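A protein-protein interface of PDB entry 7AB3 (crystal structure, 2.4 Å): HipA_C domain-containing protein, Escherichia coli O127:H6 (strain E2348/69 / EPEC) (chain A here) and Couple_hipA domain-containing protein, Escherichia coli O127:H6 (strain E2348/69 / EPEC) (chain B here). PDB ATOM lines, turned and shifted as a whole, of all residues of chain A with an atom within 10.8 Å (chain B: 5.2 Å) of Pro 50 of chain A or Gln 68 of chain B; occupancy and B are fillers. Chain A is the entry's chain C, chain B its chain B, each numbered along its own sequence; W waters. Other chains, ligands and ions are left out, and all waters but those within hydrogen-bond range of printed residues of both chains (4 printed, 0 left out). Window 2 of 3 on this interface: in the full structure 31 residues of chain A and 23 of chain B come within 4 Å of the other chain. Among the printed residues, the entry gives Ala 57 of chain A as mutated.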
ATOM      1  N   VAL A  46      -1.533  25.226  14.055  1.00  0.00           N
ATOM      2  CA  VAL A  46      -0.903  24.426  15.104  1.00  0.00           C
ATOM      3  C   VAL A  46       0.598  24.686  15.158  1.00  0.00           C
ATOM      4  O   VAL A  46       1.330  24.320  14.230  1.00  0.00           O
ATOM      5  CB  VAL A  46      -1.237  22.925  14.958  1.00  0.00           C
ATOM      6  CG1 VAL A  46      -0.626  22.113  16.088  1.00  0.00           C
ATOM      7  CG2 VAL A  46      -2.744  22.713  14.888  1.00  0.00           C
ATOM      8  N   GLN A  47       1.022  25.412  16.217  1.00  0.00           N
ATOM      9  CA  GLN A  47       2.413  25.766  16.531  1.00  0.00           C
ATOM     10  C   GLN A  47       3.165  24.525  16.993  1.00  0.00           C
ATOM     11  O   GLN A  47       2.563  23.628  17.596  1.00  0.00           O
ATOM     12  CB  GLN A  47       2.450  26.755  17.717  1.00  0.00           C
ATOM     13  CG  GLN A  47       2.569  28.231  17.376  1.00  0.00           C
ATOM     14  CD  GLN A  47       1.897  29.070  18.447  1.00  0.00           C
ATOM     15  OE1 GLN A  47       0.670  29.102  18.556  1.00  0.00           O
ATOM     16  NE2 GLN A  47       2.680  29.761  19.266  1.00  0.00           N
ATOM     17  N   GLU A  48       4.491  24.503  16.781  1.00  0.00           N
ATOM     18  CA  GLU A  48       5.293  23.390  17.282  1.00  0.00           C
ATOM     19  C   GLU A  48       5.950  23.730  18.608  1.00  0.00           C
ATOM     20  O   GLU A  48       7.021  24.339  18.634  1.00  0.00           O
ATOM     21  CB  GLU A  48       6.302  22.837  16.259  1.00  0.00           C
ATOM     22  CG  GLU A  48       5.909  21.470  15.706  1.00  0.00           C
ATOM     23  CD  GLU A  48       5.321  20.450  16.673  1.00  0.00           C
ATOM     24  OE1 GLU A  48       4.116  20.118  16.532  1.00  0.00           O
ATOM     25  OE2 GLU A  48       6.061  20.001  17.583  1.00  0.00           O
ATOM     26  N   LEU A  49       5.287  23.361  19.713  1.00  0.00           N
ATOM     27  CA  LEU A  49       5.807  23.626  21.047  1.00  0.00           C
ATOM     28  C   LEU A  49       6.900  22.627  21.384  1.00  0.00           C
ATOM     29  O   LEU A  49       6.793  21.451  21.032  1.00  0.00           O
ATOM     30  CB  LEU A  49       4.687  23.530  22.102  1.00  0.00           C
ATOM     31  CG  LEU A  49       3.414  24.332  21.879  1.00  0.00           C
ATOM     32  CD1 LEU A  49       2.500  24.203  23.053  1.00  0.00           C
ATOM     33  CD2 LEU A  49       3.698  25.781  21.639  1.00  0.00           C
ATOM     34  N   PRO A  50       7.953  23.066  22.088  1.00  0.00           N
ATOM     35  CA  PRO A  50       9.010  22.114  22.489  1.00  0.00           C
ATOM     36  C   PRO A  50       8.522  21.035  23.472  1.00  0.00           C
ATOM     37  O   PRO A  50       7.686  21.317  24.327  1.00  0.00           O
ATOM     38  CB  PRO A  50      10.060  23.003  23.166  1.00  0.00           C
ATOM     39  CG  PRO A  50       9.691  24.409  22.827  1.00  0.00           C
ATOM     40  CD  PRO A  50       8.222  24.427  22.584  1.00  0.00           C
ATOM     41  N   ARG A  51       9.062  19.804  23.366  1.00  0.00           N
ATOM     42  CA  ARG A  51       8.705  18.686  24.254  1.00  0.00           C
ATOM     43  C   ARG A  51       8.994  19.054  25.719  1.00  0.00           C
ATOM     44  O   ARG A  51      10.064  19.597  26.016  1.00  0.00           O
ATOM     45  CB  ARG A  51       9.521  17.446  23.870  1.00  0.00           C
ATOM     46  CG  ARG A  51       8.820  16.118  24.098  1.00  0.00           C
ATOM     47  CD  ARG A  51       9.720  14.964  23.671  1.00  0.00           C
ATOM     48  NE  ARG A  51       9.921  14.914  22.220  1.00  0.00           N
ATOM     49  CZ  ARG A  51      11.069  15.178  21.605  1.00  0.00           C
ATOM     50  NH1 ARG A  51      12.144  15.524  22.306  1.00  0.00           N
ATOM     51  NH2 ARG A  51      11.153  15.103  20.282  1.00  0.00           N
ATOM     52  N   GLN A  52       8.042  18.784  26.624  1.00  0.00           N
ATOM     53  CA  GLN A  52       8.221  19.125  28.037  1.00  0.00           C
ATOM     54  C   GLN A  52       9.146  18.093  28.779  1.00  0.00           C
ATOM     55  O   GLN A  52      10.376  18.248  28.783  1.00  0.00           O
ATOM     56  CB  GLN A  52       6.842  19.337  28.730  1.00  0.00           C
ATOM     57  CG  GLN A  52       5.935  20.372  28.051  1.00  0.00           C
ATOM     58  CD  GLN A  52       4.796  19.756  27.260  1.00  0.00           C
ATOM     59  OE1 GLN A  52       3.611  20.082  27.460  1.00  0.00           O
ATOM     60  NE2 GLN A  52       5.128  18.878  26.321  1.00  0.00           N
ATOM     61  N   GLN A  53       8.558  17.049  29.386  1.00  0.00           N
ATOM     62  CA  GLN A  53       9.280  15.983  30.080  1.00  0.00           C
ATOM     63  C   GLN A  53       8.532  14.655  29.843  1.00  0.00           C
ATOM     64  O   GLN A  53       7.330  14.657  29.532  1.00  0.00           O
ATOM     65  CB  GLN A  53       9.475  16.298  31.586  1.00  0.00           C
ATOM     66  CG  GLN A  53       8.254  16.038  32.479  1.00  0.00           C
ATOM     67  CD  GLN A  53       7.230  17.152  32.447  1.00  0.00           C
ATOM     68  OE1 GLN A  53       7.557  18.333  32.277  1.00  0.00           O
ATOM     69  NE2 GLN A  53       5.965  16.800  32.632  1.00  0.00           N
ATOM     70  N   LYS A  54       9.248  13.527  29.943  1.00  0.00           N
ATOM     71  CA  LYS A  54       8.692  12.180  29.713  1.00  0.00           C
ATOM     72  C   LYS A  54       7.593  11.761  30.734  1.00  0.00           C
ATOM     73  O   LYS A  54       6.797  10.848  30.461  1.00  0.00           O
ATOM     74  CB  LYS A  54       9.817  11.119  29.683  1.00  0.00           C
ATOM     75  CG  LYS A  54      11.194  11.609  29.210  1.00  0.00           C
ATOM     76  CD  LYS A  54      12.133  11.861  30.379  1.00  0.00           C
ATOM     77  CE  LYS A  54      13.535  12.159  29.915  1.00  0.00           C
ATOM     78  NZ  LYS A  54      14.464  11.026  30.185  1.00  0.00           N
ATOM     79  N   MET A  56       4.862  13.377  31.853  1.00  0.00           N
ATOM     80  CA  MET A  56       3.448  13.632  31.578  1.00  0.00           C
ATOM     81  C   MET A  56       2.858  12.642  30.573  1.00  0.00           C
ATOM     82  O   MET A  56       3.576  12.080  29.744  1.00  0.00           O
ATOM     83  CB  MET A  56       3.151  15.091  31.193  1.00  0.00           C
ATOM     84  CG  MET A  56       4.059  15.679  30.131  1.00  0.00           C
ATOM     85  SD  MET A  56       3.309  17.037  29.163  1.00  0.00           S
ATOM     86  CE  MET A  56       2.213  17.842  30.405  1.00  0.00           C
ATOM     87  N   ALA A  57       1.544  12.396  30.712  1.00  0.00           N
ATOM     88  CA  ALA A  57       0.720  11.512  29.881  1.00  0.00           C
ATOM     89  C   ALA A  57       0.593  12.044  28.463  1.00  0.00           C
ATOM     90  O   ALA A  57       0.751  13.247  28.241  1.00  0.00           O
ATOM     91  CB  ALA A  57      -0.659  11.358  30.496  1.00  0.00           C
ATOM     92  N   ILE A  58       0.321  11.150  27.497  1.00  0.00           N
ATOM     93  CA  ILE A  58       0.188  11.466  26.066  1.00  0.00           C
ATOM     94  C   ILE A  58      -0.736  12.690  25.781  1.00  0.00           C
ATOM     95  O   ILE A  58      -0.439  13.479  24.879  1.00  0.00           O
ATOM     96  CB  ILE A  58      -0.237  10.191  25.295  1.00  0.00           C
ATOM     97  CG1 ILE A  58       0.769   9.049  25.557  1.00  0.00           C
ATOM     98  CG2 ILE A  58      -0.359  10.464  23.804  1.00  0.00           C
ATOM     99  CD1 ILE A  58       0.364   7.717  25.061  1.00  0.00           C
ATOM    100  N   SEP A  59      -1.781  12.897  26.617  1.00  0.00           N
ATOM    101  CA  SEP A  59      -2.707  14.034  26.518  1.00  0.00           C
ATOM    102  CB  SEP A  59      -3.884  13.885  27.496  1.00  0.00           C
ATOM    103  OG  SEP A  59      -3.507  13.488  28.832  1.00  0.00           O
ATOM    104  C   SEP A  59      -2.029  15.420  26.680  1.00  0.00           C
ATOM    105  O   SEP A  59      -2.547  16.418  26.165  1.00  0.00           O
ATOM    106  P   SEP A  59      -4.436  14.116  29.922  1.00  0.00           P
ATOM    107  O1P SEP A  59      -4.089  13.442  31.227  1.00  0.00           O
ATOM    108  O2P SEP A  59      -5.951  13.941  29.600  1.00  0.00           O
ATOM    109  O3P SEP A  59      -4.181  15.592  30.123  1.00  0.00           O
ATOM    110  N   GLY A  60      -0.883  15.454  27.378  1.00  0.00           N
ATOM    111  CA  GLY A  60      -0.078  16.653  27.587  1.00  0.00           C
ATOM    112  C   GLY A  60       0.629  17.113  26.327  1.00  0.00           C
ATOM    113  O   GLY A  60       0.873  18.306  26.144  1.00  0.00           O
ATOM    114  N   TYR A  61       0.963  16.162  25.441  1.00  0.00           N
ATOM    115  CA  TYR A  61       1.615  16.427  24.157  1.00  0.00           C
ATOM    116  C   TYR A  61       0.640  16.727  23.027  1.00  0.00           C
ATOM    117  O   TYR A  61       1.094  17.082  21.942  1.00  0.00           O
ATOM    118  CB  TYR A  61       2.493  15.242  23.742  1.00  0.00           C
ATOM    119  CG  TYR A  61       3.502  14.829  24.785  1.00  0.00           C
ATOM    120  CD1 TYR A  61       4.530  15.681  25.164  1.00  0.00           C
ATOM    121  CD2 TYR A  61       3.428  13.589  25.399  1.00  0.00           C
ATOM    122  CE1 TYR A  61       5.470  15.301  26.117  1.00  0.00           C
ATOM    123  CE2 TYR A  61       4.365  13.193  26.345  1.00  0.00           C
ATOM    124  CZ  TYR A  61       5.394  14.047  26.694  1.00  0.00           C
ATOM    125  OH  TYR A  61       6.309  13.659  27.647  1.00  0.00           O
ATOM    126  N   GLN A  62      -0.683  16.596  23.267  1.00  0.00           N
ATOM    127  CA  GLN A  62      -1.729  16.782  22.264  1.00  0.00           C
ATOM    128  C   GLN A  62      -2.256  18.216  22.077  1.00  0.00           C
ATOM    129  O   GLN A  62      -2.923  18.774  22.957  1.00  0.00           O
ATOM    130  CB  GLN A  62      -2.918  15.838  22.535  1.00  0.00           C
ATOM    131  CG  GLN A  62      -3.987  15.886  21.447  1.00  0.00           C
ATOM    132  CD  GLN A  62      -4.490  14.518  21.125  1.00  0.00           C
ATOM    133  OE1 GLN A  62      -4.897  13.760  22.017  1.00  0.00           O
ATOM    134  NE2 GLN A  62      -4.462  14.165  19.842  1.00  0.00           N
ATOM    135  N   PRO A  63      -2.076  18.748  20.847  1.00  0.00           N
ATOM    136  CA  PRO A  63      -2.649  20.064  20.528  1.00  0.00           C
ATOM    137  C   PRO A  63      -4.181  20.055  20.419  1.00  0.00           C
ATOM    138  O   PRO A  63      -4.787  19.043  20.079  1.00  0.00           O
ATOM    139  CB  PRO A  63      -1.990  20.420  19.184  1.00  0.00           C
ATOM    140  CG  PRO A  63      -0.889  19.390  18.963  1.00  0.00           C
ATOM    141  CD  PRO A  63      -1.349  18.178  19.690  1.00  0.00           C
ATOM    142  N   LYS A  64      -4.807  21.178  20.735  1.00  0.00           N
ATOM    143  CA  LYS A  64      -6.260  21.311  20.668  1.00  0.00           C
ATOM    144  C   LYS A  64      -6.651  22.639  20.025  1.00  0.00           C
ATOM    145  O   LYS A  64      -6.201  23.705  20.453  1.00  0.00           O
ATOM    146  CB  LYS A  64      -6.908  21.156  22.056  1.00  0.00           C
ATOM    147  CG  LYS A  64      -7.238  19.708  22.379  1.00  0.00           C
ATOM    148  CD  LYS A  64      -7.331  19.445  23.861  1.00  0.00           C
ATOM    149  CE  LYS A  64      -5.961  19.296  24.485  1.00  0.00           C
ATOM    150  NZ  LYS A  64      -5.312  17.986  24.184  1.00  0.00           N
ATOM    151  N   PRO A  89      -0.280  14.199  18.160  1.00  0.00           N
ATOM    152  CA  PRO A  89       0.961  14.854  18.608  1.00  0.00           C
ATOM    153  C   PRO A  89       2.132  14.500  17.672  1.00  0.00           C
ATOM    154  O   PRO A  89       2.123  13.430  17.053  1.00  0.00           O
ATOM    155  CB  PRO A  89       1.170  14.288  20.015  1.00  0.00           C
ATOM    156  CG  PRO A  89      -0.165  13.757  20.425  1.00  0.00           C
ATOM    157  CD  PRO A  89      -0.801  13.264  19.172  1.00  0.00           C
ATOM    158  N   ALA A  90       3.124  15.391  17.530  1.00  0.00           N
ATOM    159  CA  ALA A  90       4.262  15.139  16.642  1.00  0.00           C
ATOM    160  C   ALA A  90       5.011  13.815  16.948  1.00  0.00           C
ATOM    161  O   ALA A  90       5.533  13.167  16.037  1.00  0.00           O
ATOM    162  CB  ALA A  90       5.228  16.312  16.704  1.00  0.00           C
ATOM    163  N   ASP A  91       5.030  13.405  18.219  1.00  0.00           N
ATOM    164  CA  ASP A  91       5.703  12.184  18.650  1.00  0.00           C
ATOM    165  C   ASP A  91       4.814  10.930  18.629  1.00  0.00           C
ATOM    166  O   ASP A  91       5.342   9.812  18.735  1.00  0.00           O
ATOM    167  CB  ASP A  91       6.272  12.372  20.060  1.00  0.00           C
ATOM    168  CG  ASP A  91       7.433  13.345  20.143  1.00  0.00           C
ATOM    169  OD1 ASP A  91       8.266  13.374  19.184  1.00  0.00           O
ATOM    170  OD2 ASP A  91       7.528  14.064  21.171  1.00  0.00           O
ATOM    171  N   GLY B  64      -1.896  20.941  29.951  1.00  0.00           N
ATOM    172  CA  GLY B  64      -0.865  20.489  29.032  1.00  0.00           C
ATOM    173  C   GLY B  64      -0.448  21.477  27.970  1.00  0.00           C
ATOM    174  O   GLY B  64       0.184  22.500  28.255  1.00  0.00           O
ATOM    175  N   TRP B  65      -0.774  21.127  26.718  1.00  0.00           N
ATOM    176  CA  TRP B  65      -0.447  21.868  25.504  1.00  0.00           C
ATOM    177  C   TRP B  65      -1.008  23.307  25.449  1.00  0.00           C
ATOM    178  O   TRP B  65      -0.291  24.205  25.012  1.00  0.00           O
ATOM    179  CB  TRP B  65      -0.896  21.059  24.276  1.00  0.00           C
ATOM    180  CG  TRP B  65      -0.255  21.485  22.995  1.00  0.00           C
ATOM    181  CD1 TRP B  65       0.899  21.002  22.460  1.00  0.00           C
ATOM    182  CD2 TRP B  65      -0.723  22.504  22.096  1.00  0.00           C
ATOM    183  NE1 TRP B  65       1.175  21.645  21.275  1.00  0.00           N
ATOM    184  CE2 TRP B  65       0.189  22.568  21.024  1.00  0.00           C
ATOM    185  CE3 TRP B  65      -1.859  23.322  22.063  1.00  0.00           C
ATOM    186  CZ2 TRP B  65       0.029  23.453  19.958  1.00  0.00           C
ATOM    187  CZ3 TRP B  65      -2.012  24.198  21.008  1.00  0.00           C
ATOM    188  CH2 TRP B  65      -1.075  24.257  19.970  1.00  0.00           C
ATOM    189  N   LEU B  66      -2.268  23.536  25.869  1.00  0.00           N
ATOM    190  CA  LEU B  66      -2.877  24.869  25.814  1.00  0.00           C
ATOM    191  C   LEU B  66      -2.308  25.829  26.867  1.00  0.00           C
ATOM    192  O   LEU B  66      -2.219  27.032  26.619  1.00  0.00           O
ATOM    193  CB  LEU B  66      -4.425  24.806  25.877  1.00  0.00           C
ATOM    194  CG  LEU B  66      -5.163  24.175  24.668  1.00  0.00           C
ATOM    195  CD1 LEU B  66      -6.667  24.173  24.882  1.00  0.00           C
ATOM    196  CD2 LEU B  66      -4.851  24.902  23.392  1.00  0.00           C
ATOM    197  N   ARG B  67      -1.932  25.306  28.037  1.00  0.00           N
ATOM    198  CA  ARG B  67      -1.297  26.097  29.096  1.00  0.00           C
ATOM    199  C   ARG B  67       0.160  26.427  28.694  1.00  0.00           C
ATOM    200  O   ARG B  67       0.668  27.484  29.052  1.00  0.00           O
ATOM    201  CB  ARG B  67      -1.298  25.311  30.412  1.00  0.00           C
ATOM    202  CG  ARG B  67      -0.856  26.108  31.622  1.00  0.00           C
ATOM    203  CD  ARG B  67      -0.017  25.234  32.519  1.00  0.00           C
ATOM    204  NE  ARG B  67       0.017  25.687  33.914  1.00  0.00           N
ATOM    205  CZ  ARG B  67      -0.677  25.128  34.906  1.00  0.00           C
ATOM    206  NH1 ARG B  67      -1.482  24.100  34.665  1.00  0.00           N
ATOM    207  NH2 ARG B  67      -0.560  25.584  36.146  1.00  0.00           N
ATOM    208  N   GLN B  68       0.824  25.514  27.963  1.00  0.00           N
ATOM    209  CA  GLN B  68       2.188  25.668  27.488  1.00  0.00           C
ATOM    210  C   GLN B  68       2.302  26.712  26.359  1.00  0.00           C
ATOM    211  O   GLN B  68       3.237  27.515  26.369  1.00  0.00           O
ATOM    212  CB  GLN B  68       2.706  24.319  27.009  1.00  0.00           C
ATOM    213  CG  GLN B  68       4.164  24.363  26.627  1.00  0.00           C
ATOM    214  CD  GLN B  68       4.624  23.157  25.855  1.00  0.00           C
ATOM    215  OE1 GLN B  68       3.858  22.225  25.557  1.00  0.00           O
ATOM    216  NE2 GLN B  68       5.900  23.165  25.503  1.00  0.00           N
ATOM    217  N   ARG B  69       1.355  26.696  25.390  1.00  0.00           N
ATOM    218  CA  ARG B  69       1.288  27.645  24.267  1.00  0.00           C
ATOM    219  C   ARG B  69       1.013  29.063  24.785  1.00  0.00           C
ATOM    220  O   ARG B  69       1.561  30.042  24.273  1.00  0.00           O
ATOM    221  CB  ARG B  69       0.196  27.216  23.266  1.00  0.00           C
ATOM    222  CG  ARG B  69      -0.058  28.232  22.147  1.00  0.00           C
ATOM    223  CD  ARG B  69      -1.094  27.766  21.160  1.00  0.00           C
ATOM    224  NE  ARG B  69      -2.456  27.892  21.677  1.00  0.00           N
ATOM    225  CZ  ARG B  69      -3.552  27.589  20.984  1.00  0.00           C
ATOM    226  NH1 ARG B  69      -3.457  27.145  19.736  1.00  0.00           N
ATOM    227  NH2 ARG B  69      -4.750  27.727  21.532  1.00  0.00           N
ATOM    228  N   TYR B  70       0.156  29.165  25.802  1.00  0.00           N
ATOM    229  CA  TYR B  70      -0.170  30.418  26.464  1.00  0.00           C
ATOM    230  C   TYR B  70       1.036  30.923  27.351  1.00  0.00           C
ATOM    231  O   TYR B  70       1.298  32.125  27.397  1.00  0.00           O
ATOM    232  CB  TYR B  70      -1.491  30.241  27.265  1.00  0.00           C
ATOM    233  CG  TYR B  70      -1.614  31.164  28.454  1.00  0.00           C
ATOM    234  CD1 TYR B  70      -2.019  32.482  28.294  1.00  0.00           C
ATOM    235  CD2 TYR B  70      -1.233  30.748  29.724  1.00  0.00           C
ATOM    236  CE1 TYR B  70      -2.072  33.353  29.372  1.00  0.00           C
ATOM    237  CE2 TYR B  70      -1.246  31.621  30.801  1.00  0.00           C
ATOM    238  CZ  TYR B  70      -1.669  32.924  30.624  1.00  0.00           C
ATOM    239  OH  TYR B  70      -1.700  33.787  31.693  1.00  0.00           O
ATOM    240  N   SER B  71       1.745  30.010  28.054  1.00  0.00           N
ATOM    241  CA  SER B  71       2.850  30.368  28.950  1.00  0.00           C
ATOM    242  C   SER B  71       4.098  30.867  28.266  1.00  0.00           C
ATOM    243  O   SER B  71       4.821  31.653  28.859  1.00  0.00           O
ATOM    244  CB  SER B  71       3.210  29.212  29.877  1.00  0.00           C
ATOM    245  OG  SER B  71       2.257  29.071  30.918  1.00  0.00           O
ATOM    246  N   GLN B  72       4.381  30.406  27.048  1.00  0.00           N
ATOM    247  CA  GLN B  72       5.577  30.835  26.319  1.00  0.00           C
ATOM    248  C   GLN B  72       5.471  32.269  25.776  1.00  0.00           C
ATOM    249  O   GLN B  72       6.496  32.916  25.553  1.00  0.00           O
ATOM    250  CB  GLN B  72       5.905  29.851  25.185  1.00  0.00           C
ATOM    251  CG  GLN B  72       4.773  29.687  24.185  1.00  0.00           C
ATOM    252  CD  GLN B  72       5.169  28.881  22.984  1.00  0.00           C
ATOM    253  OE1 GLN B  72       6.077  28.049  23.031  1.00  0.00           O
ATOM    254  NE2 GLN B  72       4.480  29.108  21.876  1.00  0.00           N
HETATM  255  O   HOH W   1       2.824  31.353  21.579  1.00  0.00           O
HETATM  256  O   HOH W   2      -1.255  27.014  17.745  1.00  0.00           O
HETATM  257  O   HOH W   3      -2.663  17.657  29.927  1.00  0.00           O
HETATM  258  O   HOH W   4       3.039  21.190  19.165  1.00  0.00           O
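Water W3 lies within hydrogen-bond range of O3P of SEP 59 of chain A and the backbone NH of Gly 64 of chain B. Water W1 lies within hydrogen-bond range of NE2 of Gln 72 of chain B, NE2 of Gln 47 of chain A and O of Arg 69 of chain B. Water W4 lies within hydrogen-bond range of NE1 of Trp 65 of chain B, O of Gln 47 of chain A, OE1 of Glu 48 of chain A and N of Leu 49 of chain A. Water W2 lies within hydrogen-bond range of the side-chain amide oxygen of Gln 47 of chain A and the guanidinium group of Arg 69 of chain B.
O of Gln 47 of chain A touches CZ2 of Trp 65 of chain B (3.5 Å). Gln 47 of chain A touches Arg 69 of chain B. CD1 of Leu 49 of chain A touches NE1 of Trp 65 of chain B, at 3.4 Å. Leu 49 of chain A touches Arg 69 of chain B (CD1 to N, 3.6 Å). CD2 of Leu 49 of chain A touches NE2 of Gln 72 of chain B (3.4 Å). Gly 64 of chain B touches Gly 60 of chain A. CD1 of Trp 65 of chain B touches O of Tyr 61 of chain A (3.96 Å). Trp 65 of chain B touches Gln 62 of chain A (CB to O, 3.3 Å). Trp 65 of chain B touches Pro 63 of chain A. Leu 66 of chain B touches Lys 64 of chain A (CD2 to O, 3.4 Å).
Pro 50 of chain A touches just one residue of chain B: Gln 68. No residue of chain A comes within 4 Å of Ser 71 of chain B. Of chain A, only Gln 47 and Leu 49 come within 4 Å of Gln 72 of chain B. Of the printed residues of chain B, Gln 52 of chain A touches Gln 68 (2.9 Å). Of the printed residues of chain B, Tyr 61 of chain A touches Trp 65. Printed residues of chain A within 4 Å of Leu 66 of chain B: Lys 64. Printed residues of chain B within 4 Å of Pro 63 of chain A: Trp 65. Of the printed residues of chain B, Gln 62 of chain A touches Trp 65 (3.3 Å). Tyr 70 of chain B touches none of the printed residues of chain A. Asp 91 of chain A touches none of the printed residues of chain B. The nearest residue of chain B that does not touch Pro 50 of chain A is Gln 72 of chain B (4.2 Å). The nearest printed residue of chain B that does not touch Gln 47 of chain A is Tyr 70 of chain B (7.0 Å).
The side-chain amide oxygen (OE1) of Gln 52 of chain A lies close to the side-chain sulfur (SD) of Met 56 of chain A (3.5 Å). The side-chain amino group of Lys 64 of chain A is in hydrogen-bond range of the backbone carbonyl oxygen of Gln 62 of chain A, at 2.8 Å.
Of the 21 printed residues of chain A, 9 touch a printed residue of chain B. Hydrophobic or aromatic side chains of chain A within 4 Å of the printed part of chain B: Leu 49, Pro 50 and Pro 63. Among the printed residues, no Asp or Glu carboxylate lies within 4 Å of a Lys or Arg side-chain nitrogen of the other chain.
The side-chain amide nitrogen (NE2) of Gln 68 of chain B lies within hydrogen-bond range of the backbone carbonyl oxygen (O) of Pro 50 of chain A, 2.8 Å away. The backbone carbonyl oxygen (O) of Gly 60 of chain A is in hydrogen-bond range of the backbone NH (N) of Trp 65 of chain B. OE1 of Gln 68 of chain B sits close to OE1 of Gln 52 of chain A (2.9 Å). The side-chain amide nitrogen of Gln 47 of chain A lies close to the side-chain amide nitrogen of Gln 72 of chain B (3.2 Å).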
